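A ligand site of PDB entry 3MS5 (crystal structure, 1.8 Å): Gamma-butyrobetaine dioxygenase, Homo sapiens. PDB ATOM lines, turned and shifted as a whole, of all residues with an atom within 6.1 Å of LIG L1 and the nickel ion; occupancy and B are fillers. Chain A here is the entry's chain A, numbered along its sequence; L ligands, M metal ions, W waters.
A nitrogen (N1) of LG2 L2 lies within hydrogen-bond range of the side-chain hydroxyl of Tyr 367 (3.3 Å).
An oxygen (O4) of LIG L1 is in salt-bridge range of the guanidinium group (NH1) of Arg 361, 2.8 Å away.
An oxygen (O1) of LG2 L2 sits at hydrogen-bond distance from the side-chain amide nitrogen (ND2) of Asn 192 (2.9 Å).
NH1 of Arg 350 is in salt-bridge range of O4 of LIG L1, 2.9 Å away.
NH1 of Arg 350 is in hydrogen-bond range of O of Ala 194 (3.1 Å).
The side-chain amide oxygen (OD1) of Asn 192 sits close to the backbone NH (N) of Ala 194 (3.0 Å).
The side-chain amide nitrogen (NE2) of Gln 216 lies close to the side-chain carboxylate (OD2) of Asp 205.
The backbone carbonyl oxygen of Gly 228 sits at hydrogen-bond distance from the guanidinium group of Arg 361, 2.9 Å away.
The side-chain amide nitrogen (ND2) of Asn 343 lies within hydrogen-bond range of the backbone carbonyl oxygen (O) of Asp 205, at 2.9 Å.
OD2 of Asp 205 is in hydrogen-bond range of OH of Tyr 367, at 2.6 Å.
The backbone carbonyl oxygen (O) of Arg 350 lies within hydrogen-bond range of the backbone NH (N) of Leu 200 (2.8 Å).
N of Val 184 sits at hydrogen-bond distance from O of Leu 363 (2.7 Å).
CG1 of Val 184 touches O4 of LIG L1 (3.4 Å).
CB of Ala 194 touches O1 of LIG L1, at 3.1 Å.
CD1 of Leu 200 touches C2 of LIG L1, 3.5 Å away.
CD1 of Leu 363 touches O5 of LIG L1 (3.3 Å).
Hydrophobic or aromatic side chains within 4 Å of LIG L1: Val 184, Ala 194, Leu 200, His 203, His 348 and Leu 363.
Nine residues have an atom within 4 Å of LIG L1: Val 184, Ala 194, Leu 200, His 203, Asp 205, His 348, Arg 350, Arg 361 and Leu 363.
The nickel ion is bound by O2 of LIG L1 (2.0 Å), NE2 of His 348 (2.1 Å), O3 of LIG L1 (2.1 Å), NE2 of His 203 (2.1 Å), water W1 (2.1 Å) and OD1 of Asp 205 (2.2 Å).
The nickel ion has six donor atoms within binding distance.
Water W1 bridges the side-chain amide oxygen (OE1) of Gln 216 and the side-chain carboxylate (OD2) of Asp 205.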
ATOM      1  N   TRP A 182      17.002 -12.944  -6.607  1.00  0.00           N
ATOM      2  CA  TRP A 182      17.656 -14.252  -6.744  1.00  0.00           C
ATOM      3  C   TRP A 182      18.942 -14.178  -7.524  1.00  0.00           C
ATOM      4  O   TRP A 182      19.146 -13.274  -8.357  1.00  0.00           O
ATOM      5  CB  TRP A 182      16.741 -15.298  -7.344  1.00  0.00           C
ATOM      6  CG  TRP A 182      15.741 -14.764  -8.297  1.00  0.00           C
ATOM      7  CD1 TRP A 182      14.462 -14.414  -7.963  1.00  0.00           C
ATOM      8  CD2 TRP A 182      15.858 -14.532  -9.714  1.00  0.00           C
ATOM      9  NE1 TRP A 182      13.801 -13.953  -9.066  1.00  0.00           N
ATOM     10  CE2 TRP A 182      14.607 -14.006 -10.163  1.00  0.00           C
ATOM     11  CE3 TRP A 182      16.871 -14.696 -10.656  1.00  0.00           C
ATOM     12  CZ2 TRP A 182      14.342 -13.675 -11.488  1.00  0.00           C
ATOM     13  CZ3 TRP A 182      16.619 -14.341 -11.992  1.00  0.00           C
ATOM     14  CH2 TRP A 182      15.345 -13.843 -12.388  1.00  0.00           C
ATOM     15  N   VAL A 184      21.545 -15.691 -10.126  1.00  0.00           N
ATOM     16  CA  VAL A 184      21.790 -16.654 -11.217  1.00  0.00           C
ATOM     17  C   VAL A 184      23.278 -16.906 -11.280  1.00  0.00           C
ATOM     18  O   VAL A 184      24.054 -16.082 -11.776  1.00  0.00           O
ATOM     19  CB  VAL A 184      21.297 -16.131 -12.549  1.00  0.00           C
ATOM     20  CG1 VAL A 184      21.476 -17.240 -13.660  1.00  0.00           C
ATOM     21  CG2 VAL A 184      19.796 -15.645 -12.441  1.00  0.00           C
ATOM     22  N   ASN A 192      17.475 -25.534  -9.680  1.00  0.00           N
ATOM     23  CA  ASN A 192      16.876 -25.047 -10.908  1.00  0.00           C
ATOM     24  C   ASN A 192      17.931 -25.087 -12.020  1.00  0.00           C
ATOM     25  O   ASN A 192      19.091 -24.798 -11.774  1.00  0.00           O
ATOM     26  CB  ASN A 192      16.324 -23.619 -10.704  1.00  0.00           C
ATOM     27  CG  ASN A 192      15.382 -23.170 -11.822  1.00  0.00           C
ATOM     28  OD1 ASN A 192      15.821 -22.831 -12.921  1.00  0.00           O
ATOM     29  ND2 ASN A 192      14.067 -23.131 -11.527  1.00  0.00           N
ATOM     30  N   ALA A 194      18.498 -23.144 -14.165  1.00  0.00           N
ATOM     31  CA  ALA A 194      19.091 -21.808 -14.254  1.00  0.00           C
ATOM     32  C   ALA A 194      20.432 -21.683 -13.516  1.00  0.00           C
ATOM     33  O   ALA A 194      21.330 -20.965 -13.943  1.00  0.00           O
ATOM     34  CB  ALA A 194      18.084 -20.724 -13.724  1.00  0.00           C
ATOM     35  N   TYR A 195      20.545 -22.384 -12.403  1.00  0.00           N
ATOM     36  CA  TYR A 195      21.664 -22.216 -11.475  1.00  0.00           C
ATOM     37  C   TYR A 195      22.759 -23.260 -11.809  1.00  0.00           C
ATOM     38  O   TYR A 195      23.302 -23.897 -10.913  1.00  0.00           O
ATOM     39  CB  TYR A 195      21.180 -22.327 -10.047  1.00  0.00           C
ATOM     40  CG  TYR A 195      20.114 -21.323  -9.635  1.00  0.00           C
ATOM     41  CD1 TYR A 195      19.980 -20.087 -10.283  1.00  0.00           C
ATOM     42  CD2 TYR A 195      19.255 -21.576  -8.564  1.00  0.00           C
ATOM     43  CE1 TYR A 195      19.016 -19.129  -9.881  1.00  0.00           C
ATOM     44  CE2 TYR A 195      18.259 -20.641  -8.197  1.00  0.00           C
ATOM     45  CZ  TYR A 195      18.200 -19.406  -8.847  1.00  0.00           C
ATOM     46  OH  TYR A 195      17.284 -18.445  -8.488  1.00  0.00           O
ATOM     47  N   LEU A 200      20.274 -22.279 -21.519  1.00  0.00           N
ATOM     48  CA  LEU A 200      18.821 -22.225 -21.283  1.00  0.00           C
ATOM     49  C   LEU A 200      18.224 -21.891 -22.632  1.00  0.00           C
ATOM     50  O   LEU A 200      18.615 -20.878 -23.231  1.00  0.00           O
ATOM     51  CB  LEU A 200      18.480 -21.144 -20.246  1.00  0.00           C
ATOM     52  CG  LEU A 200      19.118 -21.247 -18.848  1.00  0.00           C
ATOM     53  CD1 LEU A 200      18.642 -20.144 -17.908  1.00  0.00           C
ATOM     54  CD2 LEU A 200      18.736 -22.638 -18.279  1.00  0.00           C
ATOM     55  N   HIS A 203      12.553 -19.673 -22.928  1.00  0.00           N
ATOM     56  CA  HIS A 203      11.554 -19.924 -21.914  1.00  0.00           C
ATOM     57  C   HIS A 203      10.973 -18.591 -21.464  1.00  0.00           C
ATOM     58  O   HIS A 203      11.572 -17.514 -21.686  1.00  0.00           O
ATOM     59  CB  HIS A 203      12.121 -20.661 -20.714  1.00  0.00           C
ATOM     60  CG  HIS A 203      13.150 -19.902 -19.965  1.00  0.00           C
ATOM     61  ND1 HIS A 203      14.454 -19.804 -20.385  1.00  0.00           N
ATOM     62  CD2 HIS A 203      13.079 -19.202 -18.798  1.00  0.00           C
ATOM     63  CE1 HIS A 203      15.137 -19.073 -19.517  1.00  0.00           C
ATOM     64  NE2 HIS A 203      14.319 -18.679 -18.558  1.00  0.00           N
ATOM     65  N   THR A 204       9.785 -18.677 -20.884  1.00  0.00           N
ATOM     66  CA  THR A 204       9.245 -17.684 -19.960  1.00  0.00           C
ATOM     67  C   THR A 204       9.546 -18.160 -18.528  1.00  0.00           C
ATOM     68  O   THR A 204       9.671 -19.340 -18.269  1.00  0.00           O
ATOM     69  CB  THR A 204       7.731 -17.452 -20.181  1.00  0.00           C
ATOM     70  OG1 THR A 204       6.988 -18.635 -19.874  1.00  0.00           O
ATOM     71  CG2 THR A 204       7.406 -17.014 -21.610  1.00  0.00           C
ATOM     72  N   ASP A 205       9.728 -17.220 -17.577  1.00  0.00           N
ATOM     73  CA  ASP A 205       9.964 -17.609 -16.209  1.00  0.00           C
ATOM     74  C   ASP A 205       8.685 -17.931 -15.511  1.00  0.00           C
ATOM     75  O   ASP A 205       7.691 -17.225 -15.609  1.00  0.00           O
ATOM     76  CB  ASP A 205      10.675 -16.546 -15.420  1.00  0.00           C
ATOM     77  CG  ASP A 205      12.174 -16.621 -15.540  1.00  0.00           C
ATOM     78  OD1 ASP A 205      12.707 -17.115 -16.548  1.00  0.00           O
ATOM     79  OD2 ASP A 205      12.848 -16.157 -14.584  1.00  0.00           O
ATOM     80  N   GLN A 216      10.179  -9.017 -15.592  1.00  0.00           N
ATOM     81  CA  GLN A 216      11.420  -9.516 -15.060  1.00  0.00           C
ATOM     82  C   GLN A 216      12.485  -8.436 -15.067  1.00  0.00           C
ATOM     83  O   GLN A 216      12.616  -7.706 -16.025  1.00  0.00           O
ATOM     84  CB  GLN A 216      11.883 -10.699 -15.942  1.00  0.00           C
ATOM     85  CG  GLN A 216      12.907 -11.503 -15.292  1.00  0.00           C
ATOM     86  CD  GLN A 216      13.376 -12.688 -16.108  1.00  0.00           C
ATOM     87  OE1 GLN A 216      14.541 -12.885 -16.154  1.00  0.00           O
ATOM     88  NE2 GLN A 216      12.451 -13.493 -16.701  1.00  0.00           N
ATOM     89  N   LEU A 218      16.739  -8.128 -14.646  1.00  0.00           N
ATOM     90  CA  LEU A 218      17.963  -8.954 -14.574  1.00  0.00           C
ATOM     91  C   LEU A 218      19.179  -8.068 -14.684  1.00  0.00           C
ATOM     92  O   LEU A 218      19.356  -7.379 -15.682  1.00  0.00           O
ATOM     93  CB  LEU A 218      18.038 -10.021 -15.692  1.00  0.00           C
ATOM     94  CG  LEU A 218      17.321 -11.357 -15.654  1.00  0.00           C
ATOM     95  CD1 LEU A 218      17.636 -12.145 -16.990  1.00  0.00           C
ATOM     96  CD2 LEU A 218      17.688 -12.170 -14.445  1.00  0.00           C
ATOM     97  N   GLY A 228      27.692 -17.616 -22.217  1.00  0.00           N
ATOM     98  CA  GLY A 228      26.659 -16.886 -21.503  1.00  0.00           C
ATOM     99  C   GLY A 228      26.038 -15.672 -22.167  1.00  0.00           C
ATOM    100  O   GLY A 228      25.504 -14.806 -21.482  1.00  0.00           O
ATOM    101  N   ASP A 229      26.117 -15.599 -23.502  1.00  0.00           N
ATOM    102  CA  ASP A 229      25.377 -14.548 -24.182  1.00  0.00           C
ATOM    103  C   ASP A 229      23.878 -14.737 -24.016  1.00  0.00           C
ATOM    104  O   ASP A 229      23.382 -15.850 -23.700  1.00  0.00           O
ATOM    105  CB  ASP A 229      25.806 -14.443 -25.649  1.00  0.00           C
ATOM    106  CG  ASP A 229      27.268 -14.023 -25.804  1.00  0.00           C
ATOM    107  OD1 ASP A 229      27.876 -13.574 -24.809  1.00  0.00           O
ATOM    108  OD2 ASP A 229      27.808 -14.138 -26.925  1.00  0.00           O
ATOM    109  N   SER A 230      23.150 -13.626 -24.177  1.00  0.00           N
ATOM    110  CA  SER A 230      21.716 -13.528 -23.993  1.00  0.00           C
ATOM    111  C   SER A 230      21.007 -13.623 -25.317  1.00  0.00           C
ATOM    112  O   SER A 230      21.526 -13.166 -26.342  1.00  0.00           O
ATOM    113  CB  SER A 230      21.355 -12.194 -23.335  1.00  0.00           C
ATOM    114  OG  SER A 230      22.065 -12.024 -22.139  1.00  0.00           O
ATOM    115  N   MET A 333      25.392  -9.224 -22.127  1.00  0.00           N
ATOM    116  CA  MET A 333      25.281  -8.350 -20.943  1.00  0.00           C
ATOM    117  C   MET A 333      26.655  -8.158 -20.338  1.00  0.00           C
ATOM    118  O   MET A 333      27.400  -9.140 -20.182  1.00  0.00           O
ATOM    119  CB  MET A 333      24.310  -8.923 -19.890  1.00  0.00           C
ATOM    120  CG  MET A 333      22.857  -8.978 -20.386  1.00  0.00           C
ATOM    121  SD  MET A 333      21.691  -9.328 -19.105  1.00  0.00           S
ATOM    122  CE  MET A 333      21.741  -7.700 -18.206  1.00  0.00           C
ATOM    123  N   PHE A 341      12.038  -6.535 -18.749  1.00  0.00           N
ATOM    124  CA  PHE A 341      11.246  -7.048 -19.869  1.00  0.00           C
ATOM    125  C   PHE A 341       9.940  -7.706 -19.511  1.00  0.00           C
ATOM    126  O   PHE A 341       9.699  -8.090 -18.360  1.00  0.00           O
ATOM    127  CB  PHE A 341      12.088  -7.941 -20.791  1.00  0.00           C
ATOM    128  CG  PHE A 341      12.601  -9.205 -20.185  1.00  0.00           C
ATOM    129  CD1 PHE A 341      11.879 -10.414 -20.311  1.00  0.00           C
ATOM    130  CD2 PHE A 341      13.859  -9.236 -19.595  1.00  0.00           C
ATOM    131  CE1 PHE A 341      12.425 -11.606 -19.821  1.00  0.00           C
ATOM    132  CE2 PHE A 341      14.379 -10.406 -19.062  1.00  0.00           C
ATOM    133  CZ  PHE A 341      13.653 -11.599 -19.185  1.00  0.00           C
ATOM    134  N   ASN A 343       7.713 -10.512 -19.267  1.00  0.00           N
ATOM    135  CA  ASN A 343       7.852 -11.959 -19.068  1.00  0.00           C
ATOM    136  C   ASN A 343       6.640 -12.752 -19.570  1.00  0.00           C
ATOM    137  O   ASN A 343       6.722 -13.965 -19.740  1.00  0.00           O
ATOM    138  CB  ASN A 343       8.191 -12.281 -17.570  1.00  0.00           C
ATOM    139  CG  ASN A 343       8.440 -13.799 -17.323  1.00  0.00           C
ATOM    140  OD1 ASN A 343       9.404 -14.355 -17.913  1.00  0.00           O
ATOM    141  ND2 ASN A 343       7.556 -14.486 -16.542  1.00  0.00           N
ATOM    142  N   HIS A 348      13.084 -15.841 -23.443  1.00  0.00           N
ATOM    143  CA  HIS A 348      14.497 -15.476 -23.255  1.00  0.00           C
ATOM    144  C   HIS A 348      15.304 -16.715 -22.932  1.00  0.00           C
ATOM    145  O   HIS A 348      14.767 -17.797 -22.545  1.00  0.00           O
ATOM    146  CB  HIS A 348      14.651 -14.432 -22.161  1.00  0.00           C
ATOM    147  CG  HIS A 348      14.236 -14.932 -20.797  1.00  0.00           C
ATOM    148  ND1 HIS A 348      12.927 -15.149 -20.452  1.00  0.00           N
ATOM    149  CD2 HIS A 348      14.983 -15.347 -19.742  1.00  0.00           C
ATOM    150  CE1 HIS A 348      12.871 -15.664 -19.223  1.00  0.00           C
ATOM    151  NE2 HIS A 348      14.110 -15.810 -18.767  1.00  0.00           N
ATOM    152  N   GLY A 349      16.591 -16.570 -23.125  1.00  0.00           N
ATOM    153  CA  GLY A 349      17.495 -17.721 -22.983  1.00  0.00           C
ATOM    154  C   GLY A 349      18.927 -17.268 -22.849  1.00  0.00           C
ATOM    155  O   GLY A 349      19.247 -16.071 -22.914  1.00  0.00           O
ATOM    156  N   ARG A 350      19.836 -18.244 -22.680  1.00  0.00           N
ATOM    157  CA  ARG A 350      21.217 -17.902 -22.527  1.00  0.00           C
ATOM    158  C   ARG A 350      22.085 -19.070 -22.995  1.00  0.00           C
ATOM    159  O   ARG A 350      21.701 -20.228 -22.843  1.00  0.00           O
ATOM    160  CB  ARG A 350      21.567 -17.542 -21.070  1.00  0.00           C
ATOM    161  CG  ARG A 350      21.462 -18.640 -20.086  1.00  0.00           C
ATOM    162  CD  ARG A 350      22.744 -18.847 -19.299  1.00  0.00           C
ATOM    163  NE  ARG A 350      22.698 -20.143 -18.621  1.00  0.00           N
ATOM    164  CZ  ARG A 350      22.330 -20.357 -17.356  1.00  0.00           C
ATOM    165  NH1 ARG A 350      21.992 -19.389 -16.531  1.00  0.00           N
ATOM    166  NH2 ARG A 350      22.313 -21.601 -16.921  1.00  0.00           N
ATOM    167  N   ARG A 361      30.367 -15.964 -13.281  1.00  0.00           N
ATOM    168  CA  ARG A 361      29.175 -15.324 -13.833  1.00  0.00           C
ATOM    169  C   ARG A 361      28.099 -15.206 -12.755  1.00  0.00           C
ATOM    170  O   ARG A 361      27.790 -16.175 -12.079  1.00  0.00           O
ATOM    171  CB  ARG A 361      28.650 -16.148 -15.009  1.00  0.00           C
ATOM    172  CG  ARG A 361      27.607 -15.422 -15.830  1.00  0.00           C
ATOM    173  CD  ARG A 361      27.181 -16.315 -16.993  1.00  0.00           C
ATOM    174  NE  ARG A 361      26.270 -15.684 -17.921  1.00  0.00           N
ATOM    175  CZ  ARG A 361      24.928 -15.620 -17.843  1.00  0.00           C
ATOM    176  NH1 ARG A 361      24.223 -16.157 -16.844  1.00  0.00           N
ATOM    177  NH2 ARG A 361      24.276 -15.020 -18.840  1.00  0.00           N
ATOM    178  N   LEU A 363      24.271 -12.975 -12.187  1.00  0.00           N
ATOM    179  CA  LEU A 363      23.203 -12.013 -12.433  1.00  0.00           C
ATOM    180  C   LEU A 363      22.300 -11.989 -11.185  1.00  0.00           C
ATOM    181  O   LEU A 363      22.096 -13.040 -10.552  1.00  0.00           O
ATOM    182  CB  LEU A 363      22.351 -12.415 -13.641  1.00  0.00           C
ATOM    183  CG  LEU A 363      23.031 -12.953 -14.909  1.00  0.00           C
ATOM    184  CD1 LEU A 363      21.897 -13.215 -16.011  1.00  0.00           C
ATOM    185  CD2 LEU A 363      24.069 -11.963 -15.386  1.00  0.00           C
ATOM    186  N   TYR A 367      11.307 -10.011  -9.946  1.00  0.00           N
ATOM    187  CA  TYR A 367      10.060  -9.894 -10.673  1.00  0.00           C
ATOM    188  C   TYR A 367       9.200  -8.742 -10.167  1.00  0.00           C
ATOM    189  O   TYR A 367       9.262  -8.376  -8.983  1.00  0.00           O
ATOM    190  CB  TYR A 367       9.265 -11.191 -10.530  1.00  0.00           C
ATOM    191  CG  TYR A 367       9.972 -12.478 -10.987  1.00  0.00           C
ATOM    192  CD1 TYR A 367      10.375 -12.660 -12.308  1.00  0.00           C
ATOM    193  CD2 TYR A 367      10.182 -13.536 -10.100  1.00  0.00           C
ATOM    194  CE1 TYR A 367      11.012 -13.811 -12.716  1.00  0.00           C
ATOM    195  CE2 TYR A 367      10.779 -14.744 -10.500  1.00  0.00           C
ATOM    196  CZ  TYR A 367      11.181 -14.882 -11.825  1.00  0.00           C
ATOM    197  OH  TYR A 367      11.824 -16.046 -12.219  1.00  0.00           O
HETATM  198  C1  LIG L   1      16.829 -17.723 -15.678  1.00  0.00           C
HETATM  199  C2  LIG L   1      17.423 -16.995 -16.881  1.00  0.00           C
HETATM  200  C3  LIG L   1      19.310 -15.961 -18.041  1.00  0.00           C
HETATM  201  C4  LIG L   1      20.844 -15.892 -17.909  1.00  0.00           C
HETATM  202  O1  LIG L   1      17.565 -17.778 -14.676  1.00  0.00           O
HETATM  203  O2  LIG L   1      15.640 -18.098 -15.738  1.00  0.00           O
HETATM  204  O3  LIG L   1      16.718 -16.843 -17.851  1.00  0.00           O
HETATM  205  O4  LIG L   1      21.413 -16.591 -17.037  1.00  0.00           O
HETATM  206  N1  LIG L   1      18.706 -16.593 -16.846  1.00  0.00           N
HETATM  207  O5  LIG L   1      21.400 -15.120 -18.714  1.00  0.00           O
HETATM  208  C1  LG2 L   2      11.454 -21.045 -13.799  1.00  0.00           C
HETATM  209  N1  LG2 L   2      13.426 -18.953 -12.194  1.00  0.00           N
HETATM  210  O1  LG2 L   2      11.840 -21.849 -12.936  1.00  0.00           O
HETATM  211  C2  LG2 L   2      12.372 -19.900 -14.219  1.00  0.00           C
HETATM  212  N2  LG2 L   2      14.582 -18.554 -11.423  1.00  0.00           N
HETATM  213  O2  LG2 L   2      10.424 -21.178 -14.524  1.00  0.00           O
HETATM  214  C3  LG2 L   2      13.668 -19.654 -13.442  1.00  0.00           C
HETATM  215  C4  LG2 L   2      14.052 -17.760 -10.291  1.00  0.00           C
HETATM  216  C5  LG2 L   2      15.250 -19.753 -10.846  1.00  0.00           C
HETATM  217  C6  LG2 L   2      15.563 -17.799 -12.209  1.00  0.00           C
HETATM  218 NI    NI M   1      14.734 -17.076 -17.265  1.00  0.00          NI
HETATM  219  O   HOH W   1      15.171 -15.487 -15.952  1.00  0.00           O
